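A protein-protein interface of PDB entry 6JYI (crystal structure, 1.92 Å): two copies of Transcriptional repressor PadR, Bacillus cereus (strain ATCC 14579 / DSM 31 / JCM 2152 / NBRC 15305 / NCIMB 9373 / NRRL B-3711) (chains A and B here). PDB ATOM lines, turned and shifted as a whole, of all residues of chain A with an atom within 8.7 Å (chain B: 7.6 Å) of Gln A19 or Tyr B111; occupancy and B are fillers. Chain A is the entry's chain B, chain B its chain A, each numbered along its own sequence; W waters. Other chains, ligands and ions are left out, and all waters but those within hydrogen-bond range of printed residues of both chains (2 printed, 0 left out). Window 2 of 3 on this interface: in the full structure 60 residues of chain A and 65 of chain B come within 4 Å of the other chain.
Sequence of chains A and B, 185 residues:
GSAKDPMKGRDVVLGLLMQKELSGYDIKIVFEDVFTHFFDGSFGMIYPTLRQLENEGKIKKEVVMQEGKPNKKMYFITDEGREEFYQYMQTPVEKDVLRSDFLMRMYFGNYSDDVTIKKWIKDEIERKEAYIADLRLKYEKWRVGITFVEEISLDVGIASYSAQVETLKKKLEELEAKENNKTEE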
ATOM      1  N   VAL A  13      22.959   5.282   4.572  1.00  0.00           N
ATOM      2  CA  VAL A  13      24.325   5.782   4.509  1.00  0.00           C
ATOM      3  C   VAL A  13      25.313   4.681   4.946  1.00  0.00           C
ATOM      4  O   VAL A  13      26.328   4.459   4.287  1.00  0.00           O
ATOM      5  CB  VAL A  13      24.485   7.005   5.406  1.00  0.00           C
ATOM      6  CG1 VAL A  13      25.981   7.391   5.593  1.00  0.00           C
ATOM      7  CG2 VAL A  13      23.677   8.179   4.841  1.00  0.00           C
ATOM      8  N   LEU A  14      25.041   4.036   6.082  1.00  0.00           N
ATOM      9  CA  LEU A  14      25.945   2.991   6.586  1.00  0.00           C
ATOM     10  C   LEU A  14      26.073   1.885   5.539  1.00  0.00           C
ATOM     11  O   LEU A  14      27.176   1.445   5.243  1.00  0.00           O
ATOM     12  CB  LEU A  14      25.442   2.408   7.937  1.00  0.00           C
ATOM     13  CG  LEU A  14      25.582   3.357   9.121  1.00  0.00           C
ATOM     14  CD1 LEU A  14      24.904   2.814  10.360  1.00  0.00           C
ATOM     15  CD2 LEU A  14      27.069   3.625   9.390  1.00  0.00           C
ATOM     16  N   GLY A  15      24.950   1.462   4.956  1.00  0.00           N
ATOM     17  CA  GLY A  15      25.001   0.462   3.875  1.00  0.00           C
ATOM     18  C   GLY A  15      25.866   0.841   2.701  1.00  0.00           C
ATOM     19  O   GLY A  15      26.677   0.039   2.237  1.00  0.00           O
ATOM     20  N   LEU A  16      25.747   2.091   2.259  1.00  0.00           N
ATOM     21  CA  LEU A  16      26.630   2.608   1.209  1.00  0.00           C
ATOM     22  C   LEU A  16      28.088   2.500   1.599  1.00  0.00           C
ATOM     23  O   LEU A  16      28.917   2.240   0.749  1.00  0.00           O
ATOM     24  CB  LEU A  16      26.324   4.062   0.884  1.00  0.00           C
ATOM     25  CG  LEU A  16      25.065   4.330   0.054  1.00  0.00           C
ATOM     26  CD1 LEU A  16      24.821   5.868  -0.117  1.00  0.00           C
ATOM     27  CD2 LEU A  16      25.121   3.650  -1.303  1.00  0.00           C
ATOM     28  N   LEU A  17      28.414   2.704   2.872  1.00  0.00           N
ATOM     29  CA  LEU A  17      29.818   2.693   3.292  1.00  0.00           C
ATOM     30  C   LEU A  17      30.362   1.282   3.591  1.00  0.00           C
ATOM     31  O   LEU A  17      31.545   1.140   3.875  1.00  0.00           O
ATOM     32  CB  LEU A  17      30.015   3.599   4.527  1.00  0.00           C
ATOM     33  CG  LEU A  17      29.684   5.077   4.335  1.00  0.00           C
ATOM     34  CD1 LEU A  17      29.689   5.852   5.656  1.00  0.00           C
ATOM     35  CD2 LEU A  17      30.642   5.689   3.324  1.00  0.00           C
ATOM     36  N   MET A  18      29.505   0.259   3.576  1.00  0.00           N
ATOM     37  CA  MET A  18      29.943  -1.135   3.856  1.00  0.00           C
ATOM     38  C   MET A  18      30.998  -1.640   2.885  1.00  0.00           C
ATOM     39  O   MET A  18      31.997  -2.253   3.291  1.00  0.00           O
ATOM     40  CB  MET A  18      28.749  -2.094   3.785  1.00  0.00           C
ATOM     41  CG  MET A  18      27.740  -1.931   4.896  1.00  0.00           C
ATOM     42  SD  MET A  18      28.501  -2.583   6.550  1.00  0.00           S
ATOM     43  CE  MET A  18      28.602  -4.457   6.070  1.00  0.00           C
ATOM     44  N   GLN A  19      30.760  -1.402   1.601  1.00  0.00           N
ATOM     45  CA  GLN A  19      31.689  -1.858   0.557  1.00  0.00           C
ATOM     46  C   GLN A  19      33.036  -1.141   0.712  1.00  0.00           C
ATOM     47  O   GLN A  19      34.061  -1.771   0.779  1.00  0.00           O
ATOM     48  CB  GLN A  19      31.092  -1.606  -0.832  1.00  0.00           C
ATOM     49  N   LYS A  20      32.999   0.190   0.822  1.00  0.00           N
ATOM     50  CA  LYS A  20      34.213   1.001   0.927  1.00  0.00           C
ATOM     51  C   LYS A  20      33.869   2.432   1.318  1.00  0.00           C
ATOM     52  O   LYS A  20      32.711   2.861   1.255  1.00  0.00           O
ATOM     53  CB  LYS A  20      34.962   1.042  -0.426  1.00  0.00           C
ATOM     54  CG  LYS A  20      34.153   1.648  -1.572  1.00  0.00           C
ATOM     55  CD  LYS A  20      35.026   1.991  -2.853  1.00  0.00           C
ATOM     56  CE  LYS A  20      35.387   3.505  -2.905  1.00  0.00           C
ATOM     57  NZ  LYS A  20      35.361   4.061  -4.249  1.00  0.00           N
ATOM     58  N   GLU A  21      34.899   3.181   1.664  1.00  0.00           N
ATOM     59  CA  GLU A  21      34.747   4.578   2.035  1.00  0.00           C
ATOM     60  C   GLU A  21      34.325   5.440   0.850  1.00  0.00           C
ATOM     61  O   GLU A  21      34.691   5.152  -0.299  1.00  0.00           O
ATOM     62  CB  GLU A  21      36.063   5.100   2.618  1.00  0.00           C
ATOM     63  CG  GLU A  21      37.257   5.101   1.666  1.00  0.00           C
ATOM     64  CD  GLU A  21      37.973   3.755   1.581  1.00  0.00           C
ATOM     65  OE1 GLU A  21      37.433   2.719   2.044  1.00  0.00           O
ATOM     66  OE2 GLU A  21      39.088   3.732   1.043  1.00  0.00           O
ATOM     67  N   LEU A  22      33.588   6.513   1.139  1.00  0.00           N
ATOM     68  CA  LEU A  22      33.014   7.380   0.124  1.00  0.00           C
ATOM     69  C   LEU A  22      33.070   8.847   0.587  1.00  0.00           C
ATOM     70  O   LEU A  22      32.963   9.140   1.774  1.00  0.00           O
ATOM     71  CB  LEU A  22      31.539   7.013  -0.107  1.00  0.00           C
ATOM     72  CG  LEU A  22      31.109   5.623  -0.579  1.00  0.00           C
ATOM     73  CD1 LEU A  22      29.586   5.447  -0.532  1.00  0.00           C
ATOM     74  CD2 LEU A  22      31.651   5.370  -1.949  1.00  0.00           C
ATOM     75  N   TYR A  75      34.444   9.396   4.198  1.00  0.00           N
ATOM     76  CA  TYR A  75      33.789   8.727   5.314  1.00  0.00           C
ATOM     77  C   TYR A  75      34.056   7.217   5.289  1.00  0.00           C
ATOM     78  O   TYR A  75      33.882   6.578   4.250  1.00  0.00           O
ATOM     79  CB  TYR A  75      32.276   8.993   5.298  1.00  0.00           C
ATOM     80  CG  TYR A  75      31.943  10.457   5.356  1.00  0.00           C
ATOM     81  CD1 TYR A  75      31.909  11.134   6.573  1.00  0.00           C
ATOM     82  CD2 TYR A  75      31.687  11.182   4.191  1.00  0.00           C
ATOM     83  CE1 TYR A  75      31.593  12.491   6.634  1.00  0.00           C
ATOM     84  CE2 TYR A  75      31.389  12.527   4.244  1.00  0.00           C
ATOM     85  CZ  TYR A  75      31.353  13.183   5.472  1.00  0.00           C
ATOM     86  OH  TYR A  75      31.054  14.534   5.527  1.00  0.00           O
ATOM     87  N   ILE A  77      33.300   3.546   7.482  1.00  0.00           N
ATOM     88  CA  ILE A  77      32.433   2.922   8.477  1.00  0.00           C
ATOM     89  C   ILE A  77      33.329   2.236   9.523  1.00  0.00           C
ATOM     90  O   ILE A  77      34.442   1.814   9.202  1.00  0.00           O
ATOM     91  CB  ILE A  77      31.529   1.911   7.804  1.00  0.00           C
ATOM     92  CG1 ILE A  77      30.407   1.465   8.728  1.00  0.00           C
ATOM     93  CG2 ILE A  77      32.349   0.711   7.305  1.00  0.00           C
ATOM     94  CD1 ILE A  77      29.292   0.750   8.025  1.00  0.00           C
ATOM     95  N   ARG A  82      29.111  -0.995  11.227  1.00  0.00           N
ATOM     96  CA  ARG A  82      28.809  -2.279  10.582  1.00  0.00           C
ATOM     97  C   ARG A  82      27.759  -3.064  11.353  1.00  0.00           C
ATOM     98  O   ARG A  82      26.826  -3.606  10.760  1.00  0.00           O
ATOM     99  CB  ARG A  82      30.064  -3.141  10.402  1.00  0.00           C
ATOM    100  CG  ARG A  82      31.040  -2.593   9.393  1.00  0.00           C
ATOM    101  CD  ARG A  82      32.194  -3.577   9.101  1.00  0.00           C
ATOM    102  NE  ARG A  82      33.122  -2.969   8.163  1.00  0.00           N
ATOM    103  CZ  ARG A  82      34.176  -2.219   8.478  1.00  0.00           C
ATOM    104  NH1 ARG A  82      34.511  -1.961   9.739  1.00  0.00           N
ATOM    105  NH2 ARG A  82      34.895  -1.699   7.499  1.00  0.00           N
ATOM    106  N   PHE A  85      24.278  -1.598  10.807  1.00  0.00           N
ATOM    107  CA  PHE A  85      23.780  -1.949   9.494  1.00  0.00           C
ATOM    108  C   PHE A  85      23.283  -3.414   9.436  1.00  0.00           C
ATOM    109  O   PHE A  85      22.185  -3.708   8.941  1.00  0.00           O
ATOM    110  CB  PHE A  85      24.861  -1.758   8.452  1.00  0.00           C
ATOM    111  CG  PHE A  85      24.447  -2.248   7.124  1.00  0.00           C
ATOM    112  CD1 PHE A  85      23.584  -1.513   6.361  1.00  0.00           C
ATOM    113  CD2 PHE A  85      24.854  -3.487   6.681  1.00  0.00           C
ATOM    114  CE1 PHE A  85      23.152  -1.992   5.129  1.00  0.00           C
ATOM    115  CE2 PHE A  85      24.432  -3.973   5.473  1.00  0.00           C
ATOM    116  CZ  PHE A  85      23.587  -3.215   4.688  1.00  0.00           C
ATOM    117  N   TYR A  86      24.077  -4.336   9.972  1.00  0.00           N
ATOM    118  CA  TYR A  86      23.638  -5.735  10.007  1.00  0.00           C
ATOM    119  C   TYR A  86      22.349  -5.905  10.802  1.00  0.00           C
ATOM    120  O   TYR A  86      21.493  -6.703  10.426  1.00  0.00           O
ATOM    121  CB  TYR A  86      24.751  -6.654  10.543  1.00  0.00           C
ATOM    122  CG  TYR A  86      25.817  -6.936   9.497  1.00  0.00           C
ATOM    123  CD1 TYR A  86      25.466  -7.435   8.241  1.00  0.00           C
ATOM    124  CD2 TYR A  86      27.165  -6.688   9.750  1.00  0.00           C
ATOM    125  CE1 TYR A  86      26.432  -7.705   7.282  1.00  0.00           C
ATOM    126  CE2 TYR A  86      28.136  -6.947   8.788  1.00  0.00           C
ATOM    127  CZ  TYR A  86      27.763  -7.470   7.564  1.00  0.00           C
ATOM    128  OH  TYR A  86      28.704  -7.753   6.604  1.00  0.00           O
ATOM    129  N   TYR A  88      19.948  -3.577  11.119  1.00  0.00           N
ATOM    130  CA  TYR A  88      18.933  -3.094  10.169  1.00  0.00           C
ATOM    131  C   TYR A  88      18.525  -4.176   9.164  1.00  0.00           C
ATOM    132  O   TYR A  88      17.324  -4.403   8.953  1.00  0.00           O
ATOM    133  CB  TYR A  88      19.438  -1.844   9.461  1.00  0.00           C
ATOM    134  CG  TYR A  88      18.960  -1.640   8.037  1.00  0.00           C
ATOM    135  CD1 TYR A  88      17.652  -1.266   7.751  1.00  0.00           C
ATOM    136  CD2 TYR A  88      19.844  -1.771   6.976  1.00  0.00           C
ATOM    137  CE1 TYR A  88      17.241  -1.044   6.412  1.00  0.00           C
ATOM    138  CE2 TYR A  88      19.438  -1.579   5.676  1.00  0.00           C
ATOM    139  CZ  TYR A  88      18.137  -1.225   5.404  1.00  0.00           C
ATOM    140  OH  TYR A  88      17.811  -1.004   4.084  1.00  0.00           O
ATOM    141  N   MET A  89      19.504  -4.880   8.586  1.00  0.00           N
ATOM    142  CA  MET A  89      19.184  -5.909   7.576  1.00  0.00           C
ATOM    143  C   MET A  89      18.361  -7.073   8.152  1.00  0.00           C
ATOM    144  O   MET A  89      17.654  -7.764   7.407  1.00  0.00           O
ATOM    145  CB  MET A  89      20.452  -6.441   6.891  1.00  0.00           C
ATOM    146  CG  MET A  89      21.171  -5.435   6.034  1.00  0.00           C
ATOM    147  SD  MET A  89      20.128  -4.907   4.459  1.00  0.00           S
ATOM    148  CE  MET A  89      20.484  -6.415   3.286  1.00  0.00           C
ATOM    149  N   GLN A  90      18.456  -7.289   9.463  1.00  0.00           N
ATOM    150  CA  GLN A  90      17.688  -8.344  10.142  1.00  0.00           C
ATOM    151  C   GLN A  90      16.220  -7.962  10.396  1.00  0.00           C
ATOM    152  O   GLN A  90      15.399  -8.830  10.624  1.00  0.00           O
ATOM    153  CB  GLN A  90      18.348  -8.730  11.483  1.00  0.00           C
ATOM    154  CG  GLN A  90      19.721  -9.351  11.397  1.00  0.00           C
ATOM    155  CD  GLN A  90      19.737 -10.602  10.560  1.00  0.00           C
ATOM    156  OE1 GLN A  90      18.721 -11.283  10.417  1.00  0.00           O
ATOM    157  NE2 GLN A  90      20.896 -10.924   9.999  1.00  0.00           N
ATOM    158  N   THR A 147      25.550  -5.676  -9.889  1.00  0.00           N
ATOM    159  CA  THR A 147      25.294  -7.029  -9.434  1.00  0.00           C
ATOM    160  C   THR A 147      23.870  -7.437  -9.699  1.00  0.00           C
ATOM    161  O   THR A 147      23.006  -6.613 -10.036  1.00  0.00           O
ATOM    162  CB  THR A 147      25.595  -7.203  -7.939  1.00  0.00           C
ATOM    163  OG1 THR A 147      24.715  -6.371  -7.168  1.00  0.00           O
ATOM    164  CG2 THR A 147      27.119  -6.894  -7.637  1.00  0.00           C
ATOM    165  N   VAL A 149      21.635  -8.403  -7.575  1.00  0.00           N
ATOM    166  CA  VAL A 149      20.670  -7.836  -6.611  1.00  0.00           C
ATOM    167  C   VAL A 149      20.484  -6.339  -6.804  1.00  0.00           C
ATOM    168  O   VAL A 149      19.364  -5.853  -6.695  1.00  0.00           O
ATOM    169  CB  VAL A 149      21.009  -8.188  -5.152  1.00  0.00           C
ATOM    170  CG1 VAL A 149      20.960  -9.697  -4.982  1.00  0.00           C
ATOM    171  CG2 VAL A 149      22.395  -7.651  -4.753  1.00  0.00           C
ATOM    172  N   GLU A 150      21.559  -5.615  -7.113  1.00  0.00           N
ATOM    173  CA  GLU A 150      21.427  -4.200  -7.465  1.00  0.00           C
ATOM    174  C   GLU A 150      20.552  -4.005  -8.708  1.00  0.00           C
ATOM    175  O   GLU A 150      19.832  -3.019  -8.799  1.00  0.00           O
ATOM    176  CB  GLU A 150      22.779  -3.553  -7.713  1.00  0.00           C
ATOM    177  CG  GLU A 150      23.639  -3.402  -6.472  1.00  0.00           C
ATOM    178  CD  GLU A 150      25.064  -3.126  -6.821  1.00  0.00           C
ATOM    179  OE1 GLU A 150      25.446  -3.379  -7.995  1.00  0.00           O
ATOM    180  OE2 GLU A 150      25.835  -2.729  -5.922  1.00  0.00           O
ATOM    181  N   ARG B 105      16.728  -3.197   0.346  1.00  0.00           N
ATOM    182  CA  ARG B 105      17.274  -4.493   0.799  1.00  0.00           C
ATOM    183  C   ARG B 105      17.930  -5.205  -0.380  1.00  0.00           C
ATOM    184  O   ARG B 105      19.031  -5.753  -0.237  1.00  0.00           O
ATOM    185  CB  ARG B 105      16.209  -5.404   1.385  1.00  0.00           C
ATOM    186  CG  ARG B 105      15.422  -4.855   2.571  1.00  0.00           C
ATOM    187  CD  ARG B 105      16.251  -4.542   3.817  1.00  0.00           C
ATOM    188  NE  ARG B 105      15.353  -4.013   4.857  1.00  0.00           N
ATOM    189  CZ  ARG B 105      14.977  -4.626   5.975  1.00  0.00           C
ATOM    190  NH1 ARG B 105      15.429  -5.838   6.308  1.00  0.00           N
ATOM    191  NH2 ARG B 105      14.130  -4.002   6.794  1.00  0.00           N
ATOM    192  N   MET B 106      17.264  -5.179  -1.541  1.00  0.00           N
ATOM    193  CA  MET B 106      17.846  -5.754  -2.742  1.00  0.00           C
ATOM    194  C   MET B 106      19.122  -4.998  -3.116  1.00  0.00           C
ATOM    195  O   MET B 106      20.126  -5.617  -3.463  1.00  0.00           O
ATOM    196  CB  MET B 106      16.894  -5.733  -3.925  1.00  0.00           C
ATOM    197  CG  MET B 106      15.632  -6.512  -3.732  1.00  0.00           C
ATOM    198  SD  MET B 106      15.915  -8.411  -3.513  1.00  0.00           S
ATOM    199  CE  MET B 106      15.569  -8.530  -1.604  1.00  0.00           C
ATOM    200  N   TYR B 107      19.109  -3.671  -2.988  1.00  0.00           N
ATOM    201  CA  TYR B 107      20.297  -2.890  -3.303  1.00  0.00           C
ATOM    202  C   TYR B 107      21.510  -3.312  -2.428  1.00  0.00           C
ATOM    203  O   TYR B 107      22.637  -3.411  -2.908  1.00  0.00           O
ATOM    204  CB  TYR B 107      20.019  -1.386  -3.208  1.00  0.00           C
ATOM    205  CG  TYR B 107      21.169  -0.578  -3.716  1.00  0.00           C
ATOM    206  CD1 TYR B 107      21.378  -0.395  -5.091  1.00  0.00           C
ATOM    207  CD2 TYR B 107      22.106  -0.061  -2.840  1.00  0.00           C
ATOM    208  CE1 TYR B 107      22.499   0.319  -5.553  1.00  0.00           C
ATOM    209  CE2 TYR B 107      23.194   0.627  -3.284  1.00  0.00           C
ATOM    210  CZ  TYR B 107      23.372   0.844  -4.635  1.00  0.00           C
ATOM    211  OH  TYR B 107      24.476   1.548  -5.035  1.00  0.00           O
ATOM    212  N   PHE B 108      21.248  -3.591  -1.158  1.00  0.00           N
ATOM    213  CA  PHE B 108      22.266  -4.018  -0.225  1.00  0.00           C
ATOM    214  C   PHE B 108      22.292  -5.541  -0.103  1.00  0.00           C
ATOM    215  O   PHE B 108      22.820  -6.096   0.878  1.00  0.00           O
ATOM    216  CB  PHE B 108      22.010  -3.394   1.153  1.00  0.00           C
ATOM    217  CG  PHE B 108      22.167  -1.922   1.191  1.00  0.00           C
ATOM    218  CD1 PHE B 108      23.266  -1.313   0.614  1.00  0.00           C
ATOM    219  CD2 PHE B 108      21.210  -1.129   1.820  1.00  0.00           C
ATOM    220  CE1 PHE B 108      23.404   0.050   0.627  1.00  0.00           C
ATOM    221  CE2 PHE B 108      21.358   0.227   1.862  1.00  0.00           C
ATOM    222  CZ  PHE B 108      22.456   0.828   1.260  1.00  0.00           C
ATOM    223  N   GLY B 109      21.755  -6.227  -1.109  1.00  0.00           N
ATOM    224  CA  GLY B 109      21.605  -7.679  -1.063  1.00  0.00           C
ATOM    225  C   GLY B 109      22.888  -8.479  -0.897  1.00  0.00           C
ATOM    226  O   GLY B 109      22.891  -9.602  -0.375  1.00  0.00           O
ATOM    227  N   ASN B 110      23.996  -7.894  -1.313  1.00  0.00           N
ATOM    228  CA  ASN B 110      25.258  -8.568  -1.219  1.00  0.00           C
ATOM    229  C   ASN B 110      25.669  -8.755   0.248  1.00  0.00           C
ATOM    230  O   ASN B 110      26.480  -9.623   0.563  1.00  0.00           O
ATOM    231  CB  ASN B 110      26.279  -7.836  -2.090  1.00  0.00           C
ATOM    232  CG  ASN B 110      25.895  -7.896  -3.608  1.00  0.00           C
ATOM    233  OD1 ASN B 110      25.754  -8.991  -4.187  1.00  0.00           O
ATOM    234  ND2 ASN B 110      25.706  -6.720  -4.232  1.00  0.00           N
ATOM    235  N   TYR B 111      25.033  -8.007   1.158  1.00  0.00           N
ATOM    236  CA  TYR B 111      25.240  -8.214   2.583  1.00  0.00           C
ATOM    237  C   TYR B 111      24.241  -9.144   3.236  1.00  0.00           C
ATOM    238  O   TYR B 111      24.283  -9.350   4.451  1.00  0.00           O
ATOM    239  CB  TYR B 111      25.284  -6.874   3.283  1.00  0.00           C
ATOM    240  CG  TYR B 111      26.311  -5.988   2.644  1.00  0.00           C
ATOM    241  CD1 TYR B 111      27.662  -6.226   2.812  1.00  0.00           C
ATOM    242  CD2 TYR B 111      25.926  -4.923   1.843  1.00  0.00           C
ATOM    243  CE1 TYR B 111      28.606  -5.404   2.202  1.00  0.00           C
ATOM    244  CE2 TYR B 111      26.857  -4.102   1.243  1.00  0.00           C
ATOM    245  CZ  TYR B 111      28.185  -4.356   1.415  1.00  0.00           C
ATOM    246  OH  TYR B 111      29.089  -3.515   0.819  1.00  0.00           O
ATOM    247  N   SER B 112      23.373  -9.747   2.434  1.00  0.00           N
ATOM    248  CA  SER B 112      22.438 -10.735   2.922  1.00  0.00           C
ATOM    249  C   SER B 112      22.936 -12.145   2.483  1.00  0.00           C
ATOM    250  O   SER B 112      24.124 -12.345   2.284  1.00  0.00           O
ATOM    251  CB  SER B 112      21.057 -10.413   2.369  1.00  0.00           C
ATOM    252  OG  SER B 112      20.055 -11.208   2.983  1.00  0.00           O
ATOM    253  N   ASP B 113      22.031 -13.106   2.336  1.00  0.00           N
ATOM    254  CA  ASP B 113      22.379 -14.401   1.758  1.00  0.00           C
ATOM    255  C   ASP B 113      21.257 -14.841   0.835  1.00  0.00           C
ATOM    256  O   ASP B 113      20.183 -14.254   0.851  1.00  0.00           O
ATOM    257  CB  ASP B 113      22.602 -15.439   2.862  1.00  0.00           C
ATOM    258  CG  ASP B 113      21.353 -15.670   3.714  1.00  0.00           C
ATOM    259  OD1 ASP B 113      20.294 -16.038   3.162  1.00  0.00           O
ATOM    260  OD2 ASP B 113      21.437 -15.501   4.947  1.00  0.00           O
ATOM    261  N   ILE B 117      17.319 -13.460   0.694  1.00  0.00           N
ATOM    262  CA  ILE B 117      16.888 -12.747  -0.522  1.00  0.00           C
ATOM    263  C   ILE B 117      15.699 -13.437  -1.188  1.00  0.00           C
ATOM    264  O   ILE B 117      14.717 -12.786  -1.566  1.00  0.00           O
ATOM    265  CB  ILE B 117      18.036 -12.683  -1.568  1.00  0.00           C
ATOM    266  CG1 ILE B 117      19.201 -11.830  -1.051  1.00  0.00           C
ATOM    267  CG2 ILE B 117      17.541 -12.167  -2.893  1.00  0.00           C
ATOM    268  CD1 ILE B 117      18.796 -10.445  -0.694  1.00  0.00           C
ATOM    269  N   TRP B 120      12.573 -12.794   0.942  1.00  0.00           N
ATOM    270  CA  TRP B 120      12.096 -11.431   0.755  1.00  0.00           C
ATOM    271  C   TRP B 120      11.382 -11.254  -0.571  1.00  0.00           C
ATOM    272  O   TRP B 120      10.321 -10.607  -0.635  1.00  0.00           O
ATOM    273  CB  TRP B 120      13.272 -10.462   0.855  1.00  0.00           C
ATOM    274  CG  TRP B 120      13.704 -10.198   2.251  1.00  0.00           C
ATOM    275  CD1 TRP B 120      12.963 -10.359   3.389  1.00  0.00           C
ATOM    276  CD2 TRP B 120      14.954  -9.654   2.663  1.00  0.00           C
ATOM    277  NE1 TRP B 120      13.684  -9.952   4.478  1.00  0.00           N
ATOM    278  CE2 TRP B 120      14.908  -9.514   4.064  1.00  0.00           C
ATOM    279  CE3 TRP B 120      16.105  -9.258   1.984  1.00  0.00           C
ATOM    280  CZ2 TRP B 120      15.987  -9.012   4.810  1.00  0.00           C
ATOM    281  CZ3 TRP B 120      17.167  -8.765   2.719  1.00  0.00           C
ATOM    282  CH2 TRP B 120      17.096  -8.644   4.122  1.00  0.00           C
HETATM  283  O   HOH W   1      24.053 -10.062  -6.266  1.00  0.00           O
HETATM  284  O   HOH W   2      27.688  -1.047   0.043  1.00  0.00           O
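Among the printed residues, merely in contact across the chains: Gly A15 with Phe B108 (3.3 Å), Leu A16 with Phe B108 (3.5 Å), Met A18 with Tyr B111 (3.3 Å), Phe A85 with Phe B108 (3.9 Å), Phe A85 with Tyr B111 (3.7 Å), Tyr A86 with Tyr B111 (3.9 Å), Tyr A88 with Arg B105 (3.6 Å), Met A89 with Phe B108 (3.4 Å), Met A89 with Trp B120 (3.3 Å), Val A149 with Gly B109 (3.8 Å), Val A149 with Asn B110 (3.5 Å), Glu A150 with Met B106 (3.9 Å) and Glu A150 with Tyr B107 (3.7 Å).
Of the 11 printed residues of chain B, 8 touch a printed residue of chain A.
Printed residues of chain B that touch a printed residue of chain A: Arg B105, Met B106, Tyr B107, Phe B108, Gly B109, Asn B110, Tyr B111 and Trp B120.
Hydrophobic or aromatic side chains of chain B within 4 Å of the printed part of chain A: Met B106, Tyr B107, Phe B108, Tyr B111 and Trp B120.
Hydrophobic or aromatic side chains of chain A within 4 Å of the printed part of chain B: Met A18, Phe A85, Tyr A86, Tyr A88, Met A89 and Val A149.
Among the printed residues, 17 pairs touch across the chains.
The backbone carbonyl oxygen (O) of Val A149 lies close to the backbone carbonyl oxygen (O) of Met B106, 3.3 Å away.
OH of Tyr B111 is in hydrogen-bond range of N of Gln A19, at 2.8 Å.
ND2 of Asn B110 is in hydrogen-bond range of OG1 of Thr A147 (3.1 Å).
The guanidinium group of Arg B105 lies within hydrogen-bond range of the backbone carbonyl oxygen of Met A89 (3.1 Å).
The backbone NH (N) of Thr A147 is in hydrogen-bond range of the side-chain carboxylate (OE1) of Glu A150 (3.0 Å).
No position is printed for both chains.
Water W2 lies within hydrogen-bond range of O of Gly A15 (2.6 Å), OH of Tyr B111 (2.9 Å) and N of Gln A19 (3.5 Å).
Water W1 lies within hydrogen-bond range of the side-chain amide oxygen (OD1) of Asn B110 (2.9 Å) and the backbone NH (N) of Val A149 (3.2 Å).
Gln A19 touches one residue of chain B.
Of the printed residues of chain A, Tyr B111 touches Met A18 (3.3 Å), Gln A19 (2.8 Å), Phe A85 (3.7 Å) and Tyr A86 (3.9 Å).
Gly B109 touches just one residue of chain A: Val A149.
Printed residues of chain A within 4 Å of Met B106: Val A149 and Glu A150.
Of the printed residues of chain B, Glu A150 touches Met B106 and Tyr B107.
Of the printed residues of chain B, Met A89 touches Arg B105, Phe B108 and Trp B120.
The nearest printed residue of chain B that does not touch Val A149 is Tyr B107 (4.3 Å).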
